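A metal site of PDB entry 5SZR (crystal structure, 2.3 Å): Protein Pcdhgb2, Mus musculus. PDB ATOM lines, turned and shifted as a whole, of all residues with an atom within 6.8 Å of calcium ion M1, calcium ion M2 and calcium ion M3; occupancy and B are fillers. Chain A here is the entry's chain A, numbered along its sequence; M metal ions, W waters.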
ATOM      1  N   GLU A 121       8.934   8.688   2.188  1.00  0.00           N
ATOM      2  CA  GLU A 121       8.531   8.924   0.804  1.00  0.00           C
ATOM      3  C   GLU A 121       7.548   7.885   0.276  1.00  0.00           C
ATOM      4  O   GLU A 121       6.909   8.119  -0.747  1.00  0.00           O
ATOM      5  CB  GLU A 121       9.770   8.954  -0.097  1.00  0.00           C
ATOM      6  CG  GLU A 121      10.452   7.606  -0.263  1.00  0.00           C
ATOM      7  CD  GLU A 121      11.622   7.679  -1.209  1.00  0.00           C
ATOM      8  OE1 GLU A 121      12.666   7.061  -0.908  1.00  0.00           O
ATOM      9  OE2 GLU A 121      11.520   8.364  -2.246  1.00  0.00           O
ATOM     10  N   LEU A 173       4.673  10.414  -2.831  1.00  0.00           N
ATOM     11  CA  LEU A 173       5.859  11.223  -2.636  1.00  0.00           C
ATOM     12  C   LEU A 173       7.067  10.564  -3.300  1.00  0.00           C
ATOM     13  O   LEU A 173       7.029   9.397  -3.708  1.00  0.00           O
ATOM     14  CB  LEU A 173       6.109  11.434  -1.149  1.00  0.00           C
ATOM     15  CG  LEU A 173       4.933  12.134  -0.434  1.00  0.00           C
ATOM     16  CD1 LEU A 173       4.992  11.905   1.069  1.00  0.00           C
ATOM     17  CD2 LEU A 173       4.927  13.619  -0.749  1.00  0.00           C
ATOM     18  N   ASP A 174       8.152  11.334  -3.421  1.00  0.00           N
ATOM     19  CA  ASP A 174       9.374  10.824  -4.028  1.00  0.00           C
ATOM     20  C   ASP A 174      10.520  11.710  -3.560  1.00  0.00           C
ATOM     21  O   ASP A 174      10.670  12.832  -4.037  1.00  0.00           O
ATOM     22  CB  ASP A 174       9.270  10.802  -5.555  1.00  0.00           C
ATOM     23  CG  ASP A 174      10.536  10.277  -6.221  1.00  0.00           C
ATOM     24  OD1 ASP A 174      11.381   9.681  -5.524  1.00  0.00           O
ATOM     25  OD2 ASP A 174      10.675  10.450  -7.445  1.00  0.00           O
ATOM     26  N   ARG A 175      11.340  11.188  -2.639  1.00  0.00           N
ATOM     27  CA  ARG A 175      12.463  11.953  -2.113  1.00  0.00           C
ATOM     28  C   ARG A 175      13.433  12.325  -3.225  1.00  0.00           C
ATOM     29  O   ARG A 175      14.003  13.429  -3.207  1.00  0.00           O
ATOM     30  CB  ARG A 175      13.185  11.158  -1.023  1.00  0.00           C
ATOM     31  CG  ARG A 175      14.211  11.979  -0.275  1.00  0.00           C
ATOM     32  CD  ARG A 175      15.261  11.106   0.379  1.00  0.00           C
ATOM     33  NE  ARG A 175      16.134  10.471  -0.613  1.00  0.00           N
ATOM     34  CZ  ARG A 175      17.215  11.050  -1.133  1.00  0.00           C
ATOM     35  NH1 ARG A 175      17.549  12.267  -0.753  1.00  0.00           N
ATOM     36  NH2 ARG A 175      17.947  10.409  -2.029  1.00  0.00           N
ATOM     37  N   GLU A 176      13.645  11.424  -4.181  1.00  0.00           N
ATOM     38  CA  GLU A 176      14.600  11.694  -5.255  1.00  0.00           C
ATOM     39  C   GLU A 176      14.179  12.864  -6.131  1.00  0.00           C
ATOM     40  O   GLU A 176      15.029  13.455  -6.801  1.00  0.00           O
ATOM     41  CB  GLU A 176      14.806  10.426  -6.089  1.00  0.00           C
ATOM     42  CG  GLU A 176      15.749   9.393  -5.455  1.00  0.00           C
ATOM     43  CD  GLU A 176      15.137   8.661  -4.269  1.00  0.00           C
ATOM     44  OE1 GLU A 176      13.944   8.283  -4.346  1.00  0.00           O
ATOM     45  OE2 GLU A 176      15.843   8.462  -3.259  1.00  0.00           O
ATOM     46  N   ALA A 177      12.892  13.219  -6.142  1.00  0.00           N
ATOM     47  CA  ALA A 177      12.398  14.366  -6.893  1.00  0.00           C
ATOM     48  C   ALA A 177      12.259  15.618  -6.040  1.00  0.00           C
ATOM     49  O   ALA A 177      12.744  16.688  -6.428  1.00  0.00           O
ATOM     50  CB  ALA A 177      11.065  14.028  -7.568  1.00  0.00           C
ATOM     51  N   SER A 206      11.958  11.410   4.115  1.00  0.00           N
ATOM     52  CA  SER A 206      13.021  10.450   4.397  1.00  0.00           C
ATOM     53  C   SER A 206      13.096   9.392   3.293  1.00  0.00           C
ATOM     54  O   SER A 206      12.139   9.153   2.552  1.00  0.00           O
ATOM     55  CB  SER A 206      12.791   9.775   5.752  1.00  0.00           C
ATOM     56  OG  SER A 206      11.546   9.122   5.797  1.00  0.00           O
ATOM     57  N   ASP A 207      14.256   8.757   3.192  1.00  0.00           N
ATOM     58  CA  ASP A 207      14.566   7.893   2.053  1.00  0.00           C
ATOM     59  C   ASP A 207      14.090   6.466   2.283  1.00  0.00           C
ATOM     60  O   ASP A 207      14.103   5.952   3.414  1.00  0.00           O
ATOM     61  CB  ASP A 207      16.068   7.886   1.767  1.00  0.00           C
ATOM     62  CG  ASP A 207      16.431   7.050   0.542  1.00  0.00           C
ATOM     63  OD1 ASP A 207      15.969   7.392  -0.568  1.00  0.00           O
ATOM     64  OD2 ASP A 207      17.191   6.074   0.691  1.00  0.00           O
ATOM     65  N   VAL A 208      13.663   5.828   1.194  1.00  0.00           N
ATOM     66  CA  VAL A 208      13.346   4.406   1.131  1.00  0.00           C
ATOM     67  C   VAL A 208      14.179   3.823  -0.009  1.00  0.00           C
ATOM     68  O   VAL A 208      14.519   4.521  -0.968  1.00  0.00           O
ATOM     69  CB  VAL A 208      11.834   4.181   0.906  1.00  0.00           C
ATOM     70  CG1 VAL A 208      11.515   2.732   0.593  1.00  0.00           C
ATOM     71  CG2 VAL A 208      11.058   4.632   2.140  1.00  0.00           C
ATOM     72  N   ASN A 209      14.561   2.548   0.124  1.00  0.00           N
ATOM     73  CA  ASN A 209      15.344   1.881  -0.910  1.00  0.00           C
ATOM     74  C   ASN A 209      14.399   1.478  -2.038  1.00  0.00           C
ATOM     75  O   ASN A 209      13.964   0.321  -2.151  1.00  0.00           O
ATOM     76  CB  ASN A 209      16.091   0.680  -0.355  1.00  0.00           C
ATOM     77  CG  ASN A 209      17.061   0.082  -1.359  1.00  0.00           C
ATOM     78  OD1 ASN A 209      17.536   0.776  -2.265  1.00  0.00           O
ATOM     79  ND2 ASN A 209      17.368  -1.195  -1.203  1.00  0.00           N
ATOM     80  N   ASP A 210      14.086   2.441  -2.903  1.00  0.00           N
ATOM     81  CA  ASP A 210      13.215   2.182  -4.047  1.00  0.00           C
ATOM     82  C   ASP A 210      13.923   2.394  -5.386  1.00  0.00           C
ATOM     83  O   ASP A 210      13.258   2.519  -6.412  1.00  0.00           O
ATOM     84  CB  ASP A 210      11.950   3.047  -3.964  1.00  0.00           C
ATOM     85  CG  ASP A 210      12.261   4.532  -3.791  1.00  0.00           C
ATOM     86  OD1 ASP A 210      13.395   4.864  -3.375  1.00  0.00           O
ATOM     87  OD2 ASP A 210      11.360   5.359  -4.053  1.00  0.00           O
ATOM     88  N   ASN A 211      15.255   2.429  -5.398  1.00  0.00           N
ATOM     89  CA  ASN A 211      16.023   2.599  -6.626  1.00  0.00           C
ATOM     90  C   ASN A 211      17.087   1.523  -6.719  1.00  0.00           C
ATOM     91  O   ASN A 211      17.926   1.400  -5.832  1.00  0.00           O
ATOM     92  CB  ASN A 211      16.668   3.985  -6.693  1.00  0.00           C
ATOM     93  CG  ASN A 211      15.654   5.090  -6.929  1.00  0.00           C
ATOM     94  OD1 ASN A 211      15.278   5.358  -8.080  1.00  0.00           O
ATOM     95  ND2 ASN A 211      15.217   5.731  -5.858  1.00  0.00           N
ATOM     96  N   ALA A 212      17.042   0.749  -7.794  1.00  0.00           N
ATOM     97  CA  ALA A 212      18.064  -0.262  -8.032  1.00  0.00           C
ATOM     98  C   ALA A 212      19.303   0.387  -8.641  1.00  0.00           C
ATOM     99  O   ALA A 212      19.179   1.355  -9.414  1.00  0.00           O
ATOM    100  CB  ALA A 212      17.533  -1.351  -8.965  1.00  0.00           C
ATOM    101  N   PRO A 213      20.497  -0.079  -8.303  1.00  0.00           N
ATOM    102  CA  PRO A 213      21.699   0.415  -8.974  1.00  0.00           C
ATOM    103  C   PRO A 213      21.603   0.230 -10.482  1.00  0.00           C
ATOM    104  O   PRO A 213      20.959  -0.697 -10.975  1.00  0.00           O
ATOM    105  CB  PRO A 213      22.833  -0.428  -8.372  1.00  0.00           C
ATOM    106  CG  PRO A 213      22.152  -1.563  -7.659  1.00  0.00           C
ATOM    107  CD  PRO A 213      20.816  -1.047  -7.239  1.00  0.00           C
ATOM    108  N   ASP A 241      23.301   4.962  -7.877  1.00  0.00           N
ATOM    109  CA  ASP A 241      22.123   4.679  -7.066  1.00  0.00           C
ATOM    110  C   ASP A 241      21.717   5.938  -6.311  1.00  0.00           C
ATOM    111  O   ASP A 241      22.446   6.378  -5.407  1.00  0.00           O
ATOM    112  CB  ASP A 241      22.418   3.528  -6.105  1.00  0.00           C
ATOM    113  CG  ASP A 241      21.172   2.967  -5.435  1.00  0.00           C
ATOM    114  OD1 ASP A 241      20.379   3.742  -4.877  1.00  0.00           O
ATOM    115  OD2 ASP A 241      20.993   1.733  -5.461  1.00  0.00           O
ATOM    116  N   PRO A 242      20.574   6.558  -6.644  1.00  0.00           N
ATOM    117  CA  PRO A 242      20.243   7.863  -6.051  1.00  0.00           C
ATOM    118  C   PRO A 242      19.777   7.794  -4.610  1.00  0.00           C
ATOM    119  O   PRO A 242      19.625   8.847  -3.984  1.00  0.00           O
ATOM    120  CB  PRO A 242      19.118   8.365  -6.957  1.00  0.00           C
ATOM    121  CG  PRO A 242      18.433   7.136  -7.401  1.00  0.00           C
ATOM    122  CD  PRO A 242      19.530   6.093  -7.573  1.00  0.00           C
ATOM    123  N   ASP A 243      19.559   6.602  -4.062  1.00  0.00           N
ATOM    124  CA  ASP A 243      19.096   6.475  -2.687  1.00  0.00           C
ATOM    125  C   ASP A 243      20.195   6.911  -1.707  1.00  0.00           C
ATOM    126  O   ASP A 243      21.349   7.137  -2.084  1.00  0.00           O
ATOM    127  CB  ASP A 243      18.635   5.039  -2.410  1.00  0.00           C
ATOM    128  CG  ASP A 243      17.477   4.619  -3.304  1.00  0.00           C
ATOM    129  OD1 ASP A 243      16.689   5.498  -3.718  1.00  0.00           O
ATOM    130  OD2 ASP A 243      17.351   3.415  -3.597  1.00  0.00           O
ATOM    131  N   LEU A 244      19.826   7.012  -0.433  1.00  0.00           N
ATOM    132  CA  LEU A 244      20.697   7.588   0.582  1.00  0.00           C
ATOM    133  C   LEU A 244      21.349   6.512   1.447  1.00  0.00           C
ATOM    134  O   LEU A 244      20.769   5.462   1.719  1.00  0.00           O
ATOM    135  CB  LEU A 244      19.918   8.542   1.489  1.00  0.00           C
ATOM    136  CG  LEU A 244      19.669   9.971   1.005  1.00  0.00           C
ATOM    137  CD1 LEU A 244      18.971  10.766   2.102  1.00  0.00           C
ATOM    138  CD2 LEU A 244      20.965  10.636   0.573  1.00  0.00           C
ATOM    139  N   SER A 246      22.958   3.616   3.278  1.00  0.00           N
ATOM    140  CA  SER A 246      23.034   2.191   2.986  1.00  0.00           C
ATOM    141  C   SER A 246      22.220   1.816   1.759  1.00  0.00           C
ATOM    142  O   SER A 246      22.563   0.859   1.060  1.00  0.00           O
ATOM    143  CB  SER A 246      22.571   1.376   4.194  1.00  0.00           C
ATOM    144  OG  SER A 246      23.641   1.153   5.097  1.00  0.00           O
ATOM    145  N   ASN A 247      21.143   2.552   1.470  1.00  0.00           N
ATOM    146  CA  ASN A 247      20.336   2.252   0.298  1.00  0.00           C
ATOM    147  C   ASN A 247      21.030   2.608  -1.008  1.00  0.00           C
ATOM    148  O   ASN A 247      20.576   2.189  -2.079  1.00  0.00           O
ATOM    149  CB  ASN A 247      18.999   2.982   0.387  1.00  0.00           C
ATOM    150  CG  ASN A 247      18.197   2.593   1.614  1.00  0.00           C
ATOM    151  OD1 ASN A 247      18.403   1.533   2.195  1.00  0.00           O
ATOM    152  ND2 ASN A 247      17.282   3.460   2.015  1.00  0.00           N
ATOM    153  N   GLY A 248      22.118   3.385  -0.959  1.00  0.00           N
ATOM    154  CA  GLY A 248      22.836   3.755  -2.153  1.00  0.00           C
ATOM    155  C   GLY A 248      24.280   3.318  -2.165  1.00  0.00           C
ATOM    156  O   GLY A 248      25.067   3.742  -3.019  1.00  0.00           O
ATOM    157  N   LEU A 249      24.656   2.451  -1.226  1.00  0.00           N
ATOM    158  CA  LEU A 249      26.013   1.911  -1.146  1.00  0.00           C
ATOM    159  C   LEU A 249      26.090   0.669  -2.031  1.00  0.00           C
ATOM    160  O   LEU A 249      25.347  -0.288  -1.828  1.00  0.00           O
ATOM    161  CB  LEU A 249      26.370   1.573   0.296  1.00  0.00           C
ATOM    162  CG  LEU A 249      27.810   1.133   0.573  1.00  0.00           C
ATOM    163  CD1 LEU A 249      28.790   2.235   0.218  1.00  0.00           C
ATOM    164  CD2 LEU A 249      27.980   0.704   2.023  1.00  0.00           C
ATOM    165  N   ILE A 250      27.017   0.683  -2.997  1.00  0.00           N
ATOM    166  CA  ILE A 250      27.094  -0.346  -4.032  1.00  0.00           C
ATOM    167  C   ILE A 250      28.200  -1.340  -3.718  1.00  0.00           C
ATOM    168  O   ILE A 250      29.297  -0.963  -3.281  1.00  0.00           O
ATOM    169  CB  ILE A 250      27.334   0.280  -5.422  1.00  0.00           C
ATOM    170  CG1 ILE A 250      26.306   1.380  -5.708  1.00  0.00           C
ATOM    171  CG2 ILE A 250      27.274  -0.782  -6.506  1.00  0.00           C
ATOM    172  CD1 ILE A 250      24.902   0.867  -5.746  1.00  0.00           C
ATOM    173  N   ASP A 299      22.885  -2.945  -3.960  1.00  0.00           N
ATOM    174  CA  ASP A 299      22.898  -1.963  -2.888  1.00  0.00           C
ATOM    175  C   ASP A 299      22.761  -2.663  -1.534  1.00  0.00           C
ATOM    176  O   ASP A 299      22.528  -3.871  -1.453  1.00  0.00           O
ATOM    177  CB  ASP A 299      21.823  -0.883  -3.089  1.00  0.00           C
ATOM    178  CG  ASP A 299      20.384  -1.408  -2.947  1.00  0.00           C
ATOM    179  OD1 ASP A 299      20.119  -2.338  -2.174  1.00  0.00           O
ATOM    180  OD2 ASP A 299      19.508  -0.838  -3.629  1.00  0.00           O
ATOM    181  N   HIS A 300      22.916  -1.890  -0.461  1.00  0.00           N
ATOM    182  CA  HIS A 300      22.864  -2.413   0.901  1.00  0.00           C
ATOM    183  C   HIS A 300      21.603  -1.954   1.638  1.00  0.00           C
ATOM    184  O   HIS A 300      21.656  -1.585   2.812  1.00  0.00           O
ATOM    185  CB  HIS A 300      24.117  -2.027   1.675  1.00  0.00           C
ATOM    186  CG  HIS A 300      25.355  -2.712   1.210  1.00  0.00           C
ATOM    187  ND1 HIS A 300      25.599  -4.047   1.458  1.00  0.00           N
ATOM    188  CD2 HIS A 300      26.417  -2.260   0.500  1.00  0.00           C
ATOM    189  CE1 HIS A 300      26.767  -4.389   0.933  1.00  0.00           C
ATOM    190  NE2 HIS A 300      27.277  -3.326   0.344  1.00  0.00           N
ATOM    191  N   GLY A 301      20.459  -1.982   0.943  1.00  0.00           N
ATOM    192  CA  GLY A 301      19.184  -1.663   1.550  1.00  0.00           C
ATOM    193  C   GLY A 301      18.414  -2.911   1.960  1.00  0.00           C
ATOM    194  O   GLY A 301      18.816  -4.043   1.731  1.00  0.00           O
ATOM    195  N   LEU A 305      18.500  -4.160  -3.701  1.00  0.00           N
ATOM    196  CA  LEU A 305      18.218  -4.054  -5.126  1.00  0.00           C
ATOM    197  C   LEU A 305      19.520  -4.236  -5.896  1.00  0.00           C
ATOM    198  O   LEU A 305      20.611  -3.979  -5.375  1.00  0.00           O
ATOM    199  CB  LEU A 305      17.567  -2.709  -5.449  1.00  0.00           C
ATOM    200  CG  LEU A 305      16.173  -2.577  -4.842  1.00  0.00           C
ATOM    201  CD1 LEU A 305      15.664  -1.144  -4.968  1.00  0.00           C
ATOM    202  CD2 LEU A 305      15.215  -3.541  -5.511  1.00  0.00           C
HETATM  203 CA    CA M   1      14.813   6.444  -2.355  1.00  0.00          CA
HETATM  204 CA    CA M   2      11.744   7.589  -4.545  1.00  0.00          CA
HETATM  205 CA    CA M   3      19.087   1.744  -3.824  1.00  0.00          CA
HETATM  206  O   HOH W   1       9.438   7.544  -5.170  1.00  0.00           O
HETATM  207  O   HOH W   2      12.392   6.877  -6.866  1.00  0.00           O
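Within 4 Å of calcium ion M3: Asn 209, Asn 211, Asp 241, Asp 243, Asn 247 and Asp 299.
Calcium ion M1 is bound by OD1 of Asp 207 (2.3 Å), OD1 of Asp 210 (2.4 Å), O of Val 208 (2.4 Å), OE2 of Glu 176 (2.4 Å), OD1 of Asp 243 (2.5 Å), OE1 of Glu 121 (2.7 Å) and OE1 of Glu 176 (2.8 Å).
Calcium ion M1 has seven donor atoms within binding distance.
The side-chain carboxylate of Glu 176 sits close to the side-chain amide nitrogen of Asn 211, at 3.2 Å.
OD1 of Asp 210 lies close to ND2 of Asn 211 (3.2 Å).
The guanidinium group (NE) of Arg 175 sits close to the side-chain carboxylate (OD1) of Asp 207 (3.1 Å).
The side-chain carboxylate (OD2) of Asp 207 lies within hydrogen-bond range of the backbone NH (N) of Leu 244 (3.0 Å).
The side-chain carboxylate (OE2) of Glu 121 sits close to the backbone NH (N) of Arg 175, at 2.9 Å.
The backbone NH of Glu 121 is in hydrogen-bond range of the backbone carbonyl oxygen of Ser 206 (3.3 Å).
O of Leu 305 lies within hydrogen-bond range of N of Asp 299.
The side-chain carboxylate (OD1) of Asp 299 is in hydrogen-bond range of the backbone NH (N) of Gly 301 (3.2 Å).
Calcium ion M3 is bound by the backbone carbonyl oxygen (O) of Asn 247 (2.3 Å), the backbone carbonyl oxygen (O) of Asn 211 (2.3 Å), the side-chain amide oxygen (OD1) of Asn 209 (2.4 Å), the side-chain carboxylate (OD2) of Asp 243 (2.4 Å), the side-chain carboxylate (OD2) of Asp 241 (2.5 Å), the side-chain carboxylate (OD1) of Asp 241 (2.6 Å) and the side-chain carboxylate (OD2) of Asp 299 (2.6 Å).
Of the 27 residues printed, 4 come within 4 Å of calcium ion M2.
OE1 of Glu 176 binds calcium ion M2.
OD2 of Asp 210 binds calcium ion M2, at 2.3 Å.
The side-chain carboxylate (OD1) of Asp 174 binds calcium ion M2.
Calcium ion M2 is bound by water W1.
OE2 of Glu 121 is bound to calcium ion M2.
Water W2 is bound to calcium ion M2 (2.5 Å).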
